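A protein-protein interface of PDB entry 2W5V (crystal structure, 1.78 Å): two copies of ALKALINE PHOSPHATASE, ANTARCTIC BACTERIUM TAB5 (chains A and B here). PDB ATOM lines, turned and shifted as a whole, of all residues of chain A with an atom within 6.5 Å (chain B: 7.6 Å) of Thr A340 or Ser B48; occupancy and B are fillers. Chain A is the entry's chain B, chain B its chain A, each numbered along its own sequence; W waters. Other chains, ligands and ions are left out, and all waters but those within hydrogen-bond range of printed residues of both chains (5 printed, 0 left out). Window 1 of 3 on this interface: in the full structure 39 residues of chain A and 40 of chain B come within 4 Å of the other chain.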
ATOM      1  N   GLY A  46      26.984 -28.216  15.471  1.00  0.00           N
ATOM      2  CA  GLY A  46      27.316 -27.072  16.307  1.00  0.00           C
ATOM      3  C   GLY A  46      28.715 -26.569  15.972  1.00  0.00           C
ATOM      4  O   GLY A  46      29.359 -27.073  15.068  1.00  0.00           O
ATOM      5  N   LEU A  47      29.199 -25.576  16.700  1.00  0.00           N
ATOM      6  CA  LEU A  47      30.530 -25.049  16.421  1.00  0.00           C
ATOM      7  C   LEU A  47      31.603 -26.108  16.676  1.00  0.00           C
ATOM      8  O   LEU A  47      32.634 -26.121  16.003  1.00  0.00           O
ATOM      9  CB  LEU A  47      30.792 -23.787  17.240  1.00  0.00           C
ATOM     10  CG  LEU A  47      32.156 -23.113  17.070  1.00  0.00           C
ATOM     11  CD1 LEU A  47      32.489 -22.849  15.603  1.00  0.00           C
ATOM     12  CD2 LEU A  47      32.166 -21.821  17.875  1.00  0.00           C
ATOM     13  N   SER A  48      31.360 -27.013  17.622  1.00  0.00           N
ATOM     14  CA  SER A  48      32.323 -28.097  17.868  1.00  0.00           C
ATOM     15  C   SER A  48      32.438 -29.026  16.654  1.00  0.00           C
ATOM     16  O   SER A  48      33.537 -29.425  16.266  1.00  0.00           O
ATOM     17  CB  SER A  48      31.941 -28.893  19.113  1.00  0.00           C
ATOM     18  OG  SER A  48      32.163 -28.144  20.302  1.00  0.00           O
ATOM     19  N   ILE A  72      22.634 -17.914  15.628  1.00  0.00           N
ATOM     20  CA  ILE A  72      21.184 -18.055  15.793  1.00  0.00           C
ATOM     21  C   ILE A  72      20.770 -18.842  17.025  1.00  0.00           C
ATOM     22  O   ILE A  72      21.434 -19.805  17.433  1.00  0.00           O
ATOM     23  CB  ILE A  72      20.499 -18.692  14.552  1.00  0.00           C
ATOM     24  CG1 ILE A  72      21.188 -20.001  14.143  1.00  0.00           C
ATOM     25  CG2 ILE A  72      20.508 -17.721  13.398  1.00  0.00           C
ATOM     26  CD1 ILE A  72      20.432 -20.758  13.010  1.00  0.00           C
ATOM     27  N   LYS A  73      19.650 -18.422  17.606  1.00  0.00           N
ATOM     28  CA  LYS A  73      19.032 -19.132  18.706  1.00  0.00           C
ATOM     29  C   LYS A  73      17.967 -20.040  18.108  1.00  0.00           C
ATOM     30  O   LYS A  73      17.148 -19.587  17.307  1.00  0.00           O
ATOM     31  CB  LYS A  73      18.409 -18.140  19.689  1.00  0.00           C
ATOM     32  CG  LYS A  73      17.861 -18.831  20.935  1.00  0.00           C
ATOM     33  CD  LYS A  73      17.372 -17.851  21.986  1.00  0.00           C
ATOM     34  CE  LYS A  73      16.750 -18.616  23.156  1.00  0.00           C
ATOM     35  NZ  LYS A  73      16.214 -17.680  24.177  1.00  0.00           N
ATOM     36  N   THR A  74      17.975 -21.319  18.484  1.00  0.00           N
ATOM     37  CA  THR A  74      17.236 -22.317  17.707  1.00  0.00           C
ATOM     38  C   THR A  74      15.965 -22.887  18.340  1.00  0.00           C
ATOM     39  O   THR A  74      15.337 -23.772  17.748  1.00  0.00           O
ATOM     40  CB  THR A  74      18.137 -23.513  17.373  1.00  0.00           C
ATOM     41  OG1 THR A  74      18.571 -24.121  18.601  1.00  0.00           O
ATOM     42  CG2 THR A  74      19.358 -23.063  16.554  1.00  0.00           C
ATOM     43  N   HIS A 302      20.481 -27.013  14.489  1.00  0.00           N
ATOM     44  CA  HIS A 302      20.741 -27.223  15.915  1.00  0.00           C
ATOM     45  C   HIS A 302      22.017 -28.065  16.029  1.00  0.00           C
ATOM     46  O   HIS A 302      22.582 -28.473  15.011  1.00  0.00           O
ATOM     47  CB  HIS A 302      19.591 -27.997  16.548  1.00  0.00           C
ATOM     48  CG  HIS A 302      19.335 -29.302  15.862  1.00  0.00           C
ATOM     49  ND1 HIS A 302      20.093 -30.425  16.102  1.00  0.00           N
ATOM     50  CD2 HIS A 302      18.457 -29.633  14.889  1.00  0.00           C
ATOM     51  CE1 HIS A 302      19.672 -31.409  15.324  1.00  0.00           C
ATOM     52  NE2 HIS A 302      18.678 -30.954  14.582  1.00  0.00           N
ATOM     53  N   GLU A 303      22.467 -28.327  17.257  1.00  0.00           N
ATOM     54  CA  GLU A 303      23.630 -29.185  17.496  1.00  0.00           C
ATOM     55  C   GLU A 303      23.117 -30.553  17.919  1.00  0.00           C
ATOM     56  O   GLU A 303      21.996 -30.655  18.436  1.00  0.00           O
ATOM     57  CB  GLU A 303      24.496 -28.605  18.631  1.00  0.00           C
ATOM     58  CG  GLU A 303      25.848 -29.298  18.827  1.00  0.00           C
ATOM     59  CD  GLU A 303      25.846 -30.502  19.797  1.00  0.00           C
ATOM     60  OE1 GLU A 303      24.831 -30.769  20.492  1.00  0.00           O
ATOM     61  OE2 GLU A 303      26.893 -31.190  19.856  1.00  0.00           O
ATOM     62  N   SER A 338      20.822 -30.493  21.124  1.00  0.00           N
ATOM     63  CA  SER A 338      21.105 -29.560  22.206  1.00  0.00           C
ATOM     64  C   SER A 338      20.762 -28.142  21.761  1.00  0.00           C
ATOM     65  O   SER A 338      20.655 -27.876  20.564  1.00  0.00           O
ATOM     66  CB  SER A 338      22.567 -29.653  22.650  1.00  0.00           C
ATOM     67  OG  SER A 338      23.407 -28.969  21.742  1.00  0.00           O
ATOM     68  N   ALA A 339      20.601 -27.244  22.731  1.00  0.00           N
ATOM     69  CA  ALA A 339      20.069 -25.914  22.477  1.00  0.00           C
ATOM     70  C   ALA A 339      21.127 -24.807  22.357  1.00  0.00           C
ATOM     71  O   ALA A 339      20.795 -23.628  22.490  1.00  0.00           O
ATOM     72  CB  ALA A 339      19.030 -25.544  23.550  1.00  0.00           C
ATOM     73  N   THR A 340      22.382 -25.158  22.088  1.00  0.00           N
ATOM     74  CA  THR A 340      23.400 -24.113  21.881  1.00  0.00           C
ATOM     75  C   THR A 340      23.044 -23.209  20.709  1.00  0.00           C
ATOM     76  O   THR A 340      22.393 -23.634  19.755  1.00  0.00           O
ATOM     77  CB  THR A 340      24.805 -24.698  21.617  1.00  0.00           C
ATOM     78  OG1 THR A 340      25.725 -23.622  21.344  1.00  0.00           O
ATOM     79  CG2 THR A 340      24.764 -25.642  20.428  1.00  0.00           C
ATOM     80  N   LEU A 341      23.473 -21.951  20.787  1.00  0.00           N
ATOM     81  CA  LEU A 341      23.402 -21.072  19.633  1.00  0.00           C
ATOM     82  C   LEU A 341      24.263 -21.676  18.524  1.00  0.00           C
ATOM     83  O   LEU A 341      25.220 -22.413  18.789  1.00  0.00           O
ATOM     84  CB  LEU A 341      23.920 -19.668  19.972  1.00  0.00           C
ATOM     85  CG  LEU A 341      23.198 -18.845  21.043  1.00  0.00           C
ATOM     86  CD1 LEU A 341      23.859 -17.465  21.196  1.00  0.00           C
ATOM     87  CD2 LEU A 341      21.758 -18.681  20.706  1.00  0.00           C
ATOM     88  N   ILE A 342      23.920 -21.351  17.285  1.00  0.00           N
ATOM     89  CA  ILE A 342      24.537 -21.954  16.106  1.00  0.00           C
ATOM     90  C   ILE A 342      25.134 -20.876  15.199  1.00  0.00           C
ATOM     91  O   ILE A 342      24.485 -19.882  14.912  1.00  0.00           O
ATOM     92  CB  ILE A 342      23.457 -22.740  15.317  1.00  0.00           C
ATOM     93  CG1 ILE A 342      22.996 -23.972  16.119  1.00  0.00           C
ATOM     94  CG2 ILE A 342      23.927 -23.079  13.900  1.00  0.00           C
ATOM     95  CD1 ILE A 342      24.087 -25.021  16.333  1.00  0.00           C
ATOM     96  N   ALA B  45      34.975 -20.663  28.285  1.00  0.00           N
ATOM     97  CA  ALA B  45      33.628 -20.512  27.737  1.00  0.00           C
ATOM     98  C   ALA B  45      33.595 -20.752  26.227  1.00  0.00           C
ATOM     99  O   ALA B  45      34.033 -19.910  25.449  1.00  0.00           O
ATOM    100  CB  ALA B  45      33.079 -19.131  28.062  1.00  0.00           C
ATOM    101  N   GLY B  46      33.093 -21.910  25.814  1.00  0.00           N
ATOM    102  CA  GLY B  46      32.810 -22.147  24.408  1.00  0.00           C
ATOM    103  C   GLY B  46      31.446 -21.558  24.069  1.00  0.00           C
ATOM    104  O   GLY B  46      30.772 -20.990  24.926  1.00  0.00           O
ATOM    105  N   LEU B  47      31.011 -21.715  22.830  1.00  0.00           N
ATOM    106  CA  LEU B  47      29.707 -21.173  22.445  1.00  0.00           C
ATOM    107  C   LEU B  47      28.548 -21.790  23.255  1.00  0.00           C
ATOM    108  O   LEU B  47      27.546 -21.131  23.505  1.00  0.00           O
ATOM    109  CB  LEU B  47      29.495 -21.362  20.947  1.00  0.00           C
ATOM    110  CG  LEU B  47      28.217 -20.794  20.341  1.00  0.00           C
ATOM    111  CD1 LEU B  47      28.094 -19.298  20.654  1.00  0.00           C
ATOM    112  CD2 LEU B  47      28.242 -21.062  18.840  1.00  0.00           C
ATOM    113  N   SER B  48      28.676 -23.053  23.658  1.00  0.00           N
ATOM    114  CA  SER B  48      27.645 -23.659  24.499  1.00  0.00           C
ATOM    115  C   SER B  48      27.542 -22.942  25.849  1.00  0.00           C
ATOM    116  O   SER B  48      26.434 -22.693  26.346  1.00  0.00           O
ATOM    117  CB  SER B  48      27.909 -25.154  24.706  1.00  0.00           C
ATOM    118  OG  SER B  48      27.780 -25.858  23.480  1.00  0.00           O
ATOM    119  N   GLN B  49      28.688 -22.607  26.439  1.00  0.00           N
ATOM    120  CA  GLN B  49      28.701 -21.863  27.699  1.00  0.00           C
ATOM    121  C   GLN B  49      28.052 -20.490  27.522  1.00  0.00           C
ATOM    122  O   GLN B  49      27.189 -20.083  28.310  1.00  0.00           O
ATOM    123  CB  GLN B  49      30.139 -21.704  28.231  1.00  0.00           C
ATOM    124  CG  GLN B  49      30.703 -22.952  28.938  1.00  0.00           C
ATOM    125  CD  GLN B  49      31.356 -23.943  27.985  1.00  0.00           C
ATOM    126  OE1 GLN B  49      31.201 -23.841  26.767  1.00  0.00           O
ATOM    127  NE2 GLN B  49      32.098 -24.909  28.539  1.00  0.00           N
ATOM    128  N   ILE B  50      28.469 -19.777  26.481  1.00  0.00           N
ATOM    129  CA  ILE B  50      27.842 -18.506  26.129  1.00  0.00           C
ATOM    130  C   ILE B  50      26.323 -18.660  26.009  1.00  0.00           C
ATOM    131  O   ILE B  50      25.564 -17.860  26.557  1.00  0.00           O
ATOM    132  CB  ILE B  50      28.438 -17.952  24.813  1.00  0.00           C
ATOM    133  CG1 ILE B  50      29.888 -17.495  25.054  1.00  0.00           C
ATOM    134  CG2 ILE B  50      27.604 -16.782  24.279  1.00  0.00           C
ATOM    135  CD1 ILE B  50      30.692 -17.312  23.766  1.00  0.00           C
ATOM    136  N   SER B  51      25.888 -19.706  25.305  1.00  0.00           N
ATOM    137  CA  SER B  51      24.468 -19.944  25.059  1.00  0.00           C
ATOM    138  C   SER B  51      23.673 -20.090  26.354  1.00  0.00           C
ATOM    139  O   SER B  51      22.476 -19.829  26.377  1.00  0.00           O
ATOM    140  CB  SER B  51      24.274 -21.191  24.195  1.00  0.00           C
ATOM    141  OG  SER B  51      24.978 -21.063  22.976  1.00  0.00           O
ATOM    142  N   SER B  52      24.321 -20.507  27.438  1.00  0.00           N
ATOM    143  CA  SER B  52      23.572 -20.684  28.686  1.00  0.00           C
ATOM    144  C   SER B  52      22.943 -19.368  29.166  1.00  0.00           C
ATOM    145  O   SER B  52      21.876 -19.374  29.782  1.00  0.00           O
ATOM    146  CB  SER B  52      24.426 -21.334  29.780  1.00  0.00           C
ATOM    147  OG  SER B  52      25.463 -20.471  30.186  1.00  0.00           O
ATOM    148  N   THR B  53      23.582 -18.237  28.863  1.00  0.00           N
ATOM    149  CA  THR B  53      23.039 -16.944  29.285  1.00  0.00           C
ATOM    150  C   THR B  53      21.707 -16.648  28.592  1.00  0.00           C
ATOM    151  O   THR B  53      20.901 -15.870  29.096  1.00  0.00           O
ATOM    152  CB  THR B  53      24.021 -15.768  29.034  1.00  0.00           C
ATOM    153  OG1 THR B  53      24.164 -15.539  27.629  1.00  0.00           O
ATOM    154  CG2 THR B  53      25.389 -16.046  29.657  1.00  0.00           C
ATOM    155  N   PHE B  54      21.476 -17.265  27.434  1.00  0.00           N
ATOM    156  CA  PHE B  54      20.224 -17.050  26.712  1.00  0.00           C
ATOM    157  C   PHE B  54      19.092 -17.901  27.282  1.00  0.00           C
ATOM    158  O   PHE B  54      17.950 -17.744  26.874  1.00  0.00           O
ATOM    159  CB  PHE B  54      20.381 -17.327  25.211  1.00  0.00           C
ATOM    160  CG  PHE B  54      21.234 -16.322  24.503  1.00  0.00           C
ATOM    161  CD1 PHE B  54      22.618 -16.348  24.637  1.00  0.00           C
ATOM    162  CD2 PHE B  54      20.661 -15.328  23.729  1.00  0.00           C
ATOM    163  CE1 PHE B  54      23.415 -15.409  23.990  1.00  0.00           C
ATOM    164  CE2 PHE B  54      21.454 -14.389  23.082  1.00  0.00           C
ATOM    165  CZ  PHE B  54      22.831 -14.433  23.218  1.00  0.00           C
ATOM    166  N   TYR B  55      19.410 -18.798  28.216  1.00  0.00           N
ATOM    167  CA  TYR B  55      18.384 -19.644  28.841  1.00  0.00           C
ATOM    168  C   TYR B  55      18.308 -19.541  30.366  1.00  0.00           C
ATOM    169  O   TYR B  55      17.255 -19.794  30.954  1.00  0.00           O
ATOM    170  CB  TYR B  55      18.552 -21.121  28.442  1.00  0.00           C
ATOM    171  CG  TYR B  55      18.373 -21.364  26.964  1.00  0.00           C
ATOM    172  CD1 TYR B  55      19.464 -21.368  26.110  1.00  0.00           C
ATOM    173  CD2 TYR B  55      17.109 -21.562  26.418  1.00  0.00           C
ATOM    174  CE1 TYR B  55      19.307 -21.564  24.755  1.00  0.00           C
ATOM    175  CE2 TYR B  55      16.940 -21.770  25.057  1.00  0.00           C
ATOM    176  CZ  TYR B  55      18.044 -21.763  24.232  1.00  0.00           C
ATOM    177  OH  TYR B  55      17.897 -21.968  22.883  1.00  0.00           O
ATOM    178  N   PHE B  56      19.416 -19.186  31.006  1.00  0.00           N
ATOM    179  CA  PHE B  56      19.501 -19.244  32.466  1.00  0.00           C
ATOM    180  C   PHE B  56      19.787 -17.892  33.123  1.00  0.00           C
ATOM    181  O   PHE B  56      20.137 -17.831  34.299  1.00  0.00           O
ATOM    182  CB  PHE B  56      20.558 -20.271  32.894  1.00  0.00           C
ATOM    183  CG  PHE B  56      20.228 -21.680  32.487  1.00  0.00           C
ATOM    184  CD1 PHE B  56      20.793 -22.243  31.351  1.00  0.00           C
ATOM    185  CD2 PHE B  56      19.338 -22.440  33.233  1.00  0.00           C
ATOM    186  CE1 PHE B  56      20.481 -23.548  30.964  1.00  0.00           C
ATOM    187  CE2 PHE B  56      19.023 -23.738  32.853  1.00  0.00           C
ATOM    188  CZ  PHE B  56      19.597 -24.292  31.713  1.00  0.00           C
ATOM    189  N   LEU B 270      29.137 -23.066  36.844  1.00  0.00           N
ATOM    190  CA  LEU B 270      29.516 -22.524  35.547  1.00  0.00           C
ATOM    191  C   LEU B 270      28.553 -21.410  35.127  1.00  0.00           C
ATOM    192  O   LEU B 270      28.973 -20.323  34.714  1.00  0.00           O
ATOM    193  CB  LEU B 270      29.521 -23.650  34.510  1.00  0.00           C
ATOM    194  CG  LEU B 270      30.000 -23.360  33.093  1.00  0.00           C
ATOM    195  CD1 LEU B 270      30.304 -24.687  32.388  1.00  0.00           C
ATOM    196  CD2 LEU B 270      28.935 -22.597  32.338  1.00  0.00           C
ATOM    197  N   ILE B 274      29.281 -17.451  34.429  1.00  0.00           N
ATOM    198  CA  ILE B 274      29.206 -16.793  33.128  1.00  0.00           C
ATOM    199  C   ILE B 274      28.140 -15.698  33.075  1.00  0.00           C
ATOM    200  O   ILE B 274      28.269 -14.769  32.290  1.00  0.00           O
ATOM    201  CB  ILE B 274      29.053 -17.763  31.941  1.00  0.00           C
ATOM    202  CG1 ILE B 274      29.398 -17.025  30.642  1.00  0.00           C
ATOM    203  CG2 ILE B 274      27.663 -18.350  31.893  1.00  0.00           C
ATOM    204  CD1 ILE B 274      29.571 -17.928  29.441  1.00  0.00           C
ATOM    205  N   GLU B 303      37.491 -23.858  25.405  1.00  0.00           N
ATOM    206  CA  GLU B 303      36.274 -24.394  26.015  1.00  0.00           C
ATOM    207  C   GLU B 303      36.696 -25.368  27.100  1.00  0.00           C
ATOM    208  O   GLU B 303      37.788 -25.927  27.035  1.00  0.00           O
ATOM    209  CB  GLU B 303      35.464 -25.168  24.962  1.00  0.00           C
ATOM    210  CG  GLU B 303      34.010 -25.467  25.335  1.00  0.00           C
ATOM    211  CD  GLU B 303      33.819 -26.782  26.111  1.00  0.00           C
ATOM    212  OE1 GLU B 303      34.726 -27.642  26.117  1.00  0.00           O
ATOM    213  OE2 GLU B 303      32.737 -26.958  26.712  1.00  0.00           O
ATOM    214  N   GLY B 306      33.160 -29.835  27.840  1.00  0.00           N
ATOM    215  CA  GLY B 306      32.200 -30.308  26.853  1.00  0.00           C
ATOM    216  C   GLY B 306      30.772 -29.964  27.266  1.00  0.00           C
ATOM    217  O   GLY B 306      29.826 -30.696  26.960  1.00  0.00           O
ATOM    218  N   PHE B 307      30.620 -28.842  27.968  1.00  0.00           N
ATOM    219  CA  PHE B 307      29.306 -28.343  28.392  1.00  0.00           C
ATOM    220  C   PHE B 307      28.313 -28.342  27.223  1.00  0.00           C
ATOM    221  O   PHE B 307      28.631 -27.870  26.127  1.00  0.00           O
ATOM    222  CB  PHE B 307      29.472 -26.937  28.993  1.00  0.00           C
ATOM    223  CG  PHE B 307      28.193 -26.306  29.477  1.00  0.00           C
ATOM    224  CD1 PHE B 307      27.633 -26.677  30.687  1.00  0.00           C
ATOM    225  CD2 PHE B 307      27.579 -25.305  28.735  1.00  0.00           C
ATOM    226  CE1 PHE B 307      26.460 -26.074  31.138  1.00  0.00           C
ATOM    227  CE2 PHE B 307      26.413 -24.697  29.172  1.00  0.00           C
ATOM    228  CZ  PHE B 307      25.847 -25.085  30.372  1.00  0.00           C
ATOM    229  N   THR B 308      27.115 -28.876  27.470  1.00  0.00           N
ATOM    230  CA  THR B 308      26.104 -29.101  26.423  1.00  0.00           C
ATOM    231  C   THR B 308      24.710 -28.794  26.966  1.00  0.00           C
ATOM    232  O   THR B 308      24.360 -29.242  28.065  1.00  0.00           O
ATOM    233  CB  THR B 308      26.139 -30.577  25.949  1.00  0.00           C
ATOM    234  OG1 THR B 308      27.409 -30.853  25.356  1.00  0.00           O
ATOM    235  CG2 THR B 308      25.035 -30.872  24.923  1.00  0.00           C
ATOM    236  N   LEU B 309      23.917 -28.025  26.215  1.00  0.00           N
ATOM    237  CA  LEU B 309      22.552 -27.705  26.640  1.00  0.00           C
ATOM    238  C   LEU B 309      21.610 -28.800  26.153  1.00  0.00           C
ATOM    239  O   LEU B 309      20.738 -28.576  25.310  1.00  0.00           O
ATOM    240  CB  LEU B 309      22.113 -26.325  26.129  1.00  0.00           C
ATOM    241  CG  LEU B 309      22.967 -25.152  26.638  1.00  0.00           C
ATOM    242  CD1 LEU B 309      22.652 -23.875  25.879  1.00  0.00           C
ATOM    243  CD2 LEU B 309      22.782 -24.933  28.131  1.00  0.00           C
ATOM    244  N   ALA B 310      21.805 -29.992  26.696  1.00  0.00           N
ATOM    245  CA  ALA B 310      21.068 -31.163  26.255  1.00  0.00           C
ATOM    246  C   ALA B 310      19.629 -31.125  26.739  1.00  0.00           C
ATOM    247  O   ALA B 310      19.287 -30.371  27.649  1.00  0.00           O
ATOM    248  CB  ALA B 310      21.760 -32.428  26.763  1.00  0.00           C
ATOM    249  N   ILE B 328      15.832 -27.897  29.183  1.00  0.00           N
ATOM    250  CA  ILE B 328      17.260 -28.163  29.089  1.00  0.00           C
ATOM    251  C   ILE B 328      17.814 -28.787  30.371  1.00  0.00           C
ATOM    252  O   ILE B 328      17.472 -28.369  31.478  1.00  0.00           O
ATOM    253  CB  ILE B 328      18.028 -26.863  28.788  1.00  0.00           C
ATOM    254  CG1 ILE B 328      17.710 -26.377  27.373  1.00  0.00           C
ATOM    255  CG2 ILE B 328      19.540 -27.057  29.008  1.00  0.00           C
ATOM    256  CD1 ILE B 328      17.986 -24.896  27.170  1.00  0.00           C
ATOM    257  N   THR B 331      24.745 -30.857  30.486  1.00  0.00           N
ATOM    258  CA  THR B 331      25.592 -32.031  30.684  1.00  0.00           C
ATOM    259  C   THR B 331      27.032 -31.749  30.272  1.00  0.00           C
ATOM    260  O   THR B 331      27.324 -30.725  29.637  1.00  0.00           O
ATOM    261  CB  THR B 331      25.061 -33.262  29.901  1.00  0.00           C
ATOM    262  OG1 THR B 331      25.081 -32.989  28.494  1.00  0.00           O
ATOM    263  CG2 THR B 331      23.637 -33.587  30.315  1.00  0.00           C
ATOM    264  N   THR B 340      37.625 -26.864  20.447  1.00  0.00           N
ATOM    265  CA  THR B 340      36.683 -26.213  19.542  1.00  0.00           C
ATOM    266  C   THR B 340      37.136 -24.784  19.226  1.00  0.00           C
ATOM    267  O   THR B 340      37.793 -24.133  20.055  1.00  0.00           O
ATOM    268  CB  THR B 340      35.270 -26.175  20.137  1.00  0.00           C
ATOM    269  OG1 THR B 340      34.392 -25.465  19.239  1.00  0.00           O
ATOM    270  CG2 THR B 340      35.272 -25.484  21.500  1.00  0.00           C
ATOM    271  N   PRO B 343      34.227 -18.234  19.792  1.00  0.00           N
ATOM    272  CA  PRO B 343      33.721 -16.956  19.269  1.00  0.00           C
ATOM    273  C   PRO B 343      34.491 -15.744  19.792  1.00  0.00           C
ATOM    274  O   PRO B 343      34.894 -15.718  20.957  1.00  0.00           O
ATOM    275  CB  PRO B 343      32.277 -16.895  19.806  1.00  0.00           C
ATOM    276  CG  PRO B 343      31.927 -18.295  20.161  1.00  0.00           C
ATOM    277  CD  PRO B 343      33.215 -18.943  20.593  1.00  0.00           C
HETATM  278  O   HOH W   1      24.966 -27.365  23.670  1.00  0.00           O
HETATM  279  O   HOH W   2      14.821 -18.648  26.510  1.00  0.00           O
HETATM  280  O   HOH W   3      28.630 -25.160  20.817  1.00  0.00           O
HETATM  281  O   HOH W   4      19.724 -21.665  20.614  1.00  0.00           O
HETATM  282  O   HOH W   5      31.385 -25.330  20.727  1.00  0.00           O
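Leu A47 touches Thr B340, and with the chains exchanged Thr A340 touches Leu B47.
Ser A48 touches Thr B340, and with the chains exchanged Thr A340 touches Ser B48.
Positions printed for both chains: 46, 47, 48, 303 and 340.
The side-chain hydroxyl of Ser B51 is in hydrogen-bond range of the side-chain hydroxyl of Thr A340 (3.1 Å).
The side-chain hydroxyl (OG) of Ser B51 is in hydrogen-bond range of the backbone NH (N) of Leu A341, at 2.8 Å.
The side-chain amino group (NZ) of Lys A73 lies within hydrogen-bond range of the backbone carbonyl oxygen (O) of Phe B54, 3.2 Å away.
The side-chain hydroxyl (OH) of Tyr B55 sits at hydrogen-bond distance from the backbone carbonyl oxygen (O) of Ala A339, 3.4 Å away.
O of Leu B309 lies within hydrogen-bond range of N of Ala A339 (2.9 Å).
Printed residues of chain B within 4 Å of Thr A340: Leu B47, Ser B48 and Ser B51.
Printed residues of chain A within 4 Å of Thr B308: Ser A338.
Of the printed residues of chain A, Tyr B55 touches Lys A73 (3.6 Å) and Ala A339 (3.4 Å).
Printed residues of chain A within 4 Å of Leu B47: Thr A340 (3.8 Å) and Leu A341 (3.3 Å).
Of the printed residues of chain A, Ser B51 touches Thr A340 and Leu A341.
Of the printed residues of chain A, Ile B328 touches Ala A339 (3.8 Å).
Phe B307 touches none of the printed residues of chain A.
The nearest printed residue of chain B that does not touch Thr A340 is Leu B309 (4.01 Å).
The nearest printed residue of chain B that does not touch Ser A48 is Ser B48 (5.9 Å).
Hydrophobic or aromatic side chains of chain A that line the printed part of chain B: Leu A47, Ala A339 and Leu A341.
Of the 24 printed residues of chain B, 9 touch a printed residue of chain A.
Hydrophobic or aromatic side chains of chain B within 4 Å of the printed part of chain A: Leu B47, Phe B54, Tyr B55, Leu B309 and Ile B328.
Among the printed residues, 15 pairs touch across the chains.
Among the printed residues, no Asp or Glu carboxylate lies within 4 Å of a Lys or Arg side-chain nitrogen of the other chain.
The backbone carbonyl oxygen (O) of Leu B47 is in hydrogen-bond range of the side-chain hydroxyl (OG) of Ser B51, at 2.6 Å.
The side-chain hydroxyl of Ser B48 sits close to the backbone carbonyl oxygen of Phe B307 (3.4 Å).
The backbone carbonyl oxygen of Gly B306 is in hydrogen-bond range of the side-chain hydroxyl of Thr B308.
The backbone NH (N) of Thr B308 is in hydrogen-bond range of the backbone carbonyl oxygen (O) of Thr B331 (2.9 Å).
The side-chain carboxylate (OE1) of Glu A303 lies within hydrogen-bond range of the side-chain hydroxyl (OG) of Ser A338 (2.6 Å).
Water W4 lies within hydrogen-bond range of the backbone NH (N) of Thr A74 (2.8 Å), the backbone carbonyl oxygen (O) of Ala A339 (2.9 Å), the side-chain hydroxyl (OH) of Tyr B55 (2.9 Å) and the backbone carbonyl oxygen (O) of Thr A340 (3.4 Å).
Water W1 lies within hydrogen-bond range of N of Leu B309, OG of Ser A338 and OG of Ser B48.
Water W3 lies within hydrogen-bond range of the side-chain hydroxyl of Ser B48 (2.9 Å) and the side-chain hydroxyl of Thr A340 (3.3 Å).
Water W2 lies within hydrogen-bond range of the side-chain amino group (NZ) of Lys A73 and the backbone carbonyl oxygen (O) of Phe B54.
Water W5 lies within hydrogen-bond range of the side-chain hydroxyl of Ser A48 (3.0 Å) and the side-chain hydroxyl of Thr B340 (3.4 Å).
Among the printed residues, merely in contact across the chains: Leu A47 with Thr B340, Ser A48 with Thr B340, Lys A73 with Tyr B55, Ser A338 with Thr B308, Ser A338 with Leu B309, Ala A339 with Ile B328, Thr A340 with Leu B47, Thr A340 with Ser B48, Leu A341 with Leu B47 and Leu A341 with Phe B54.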
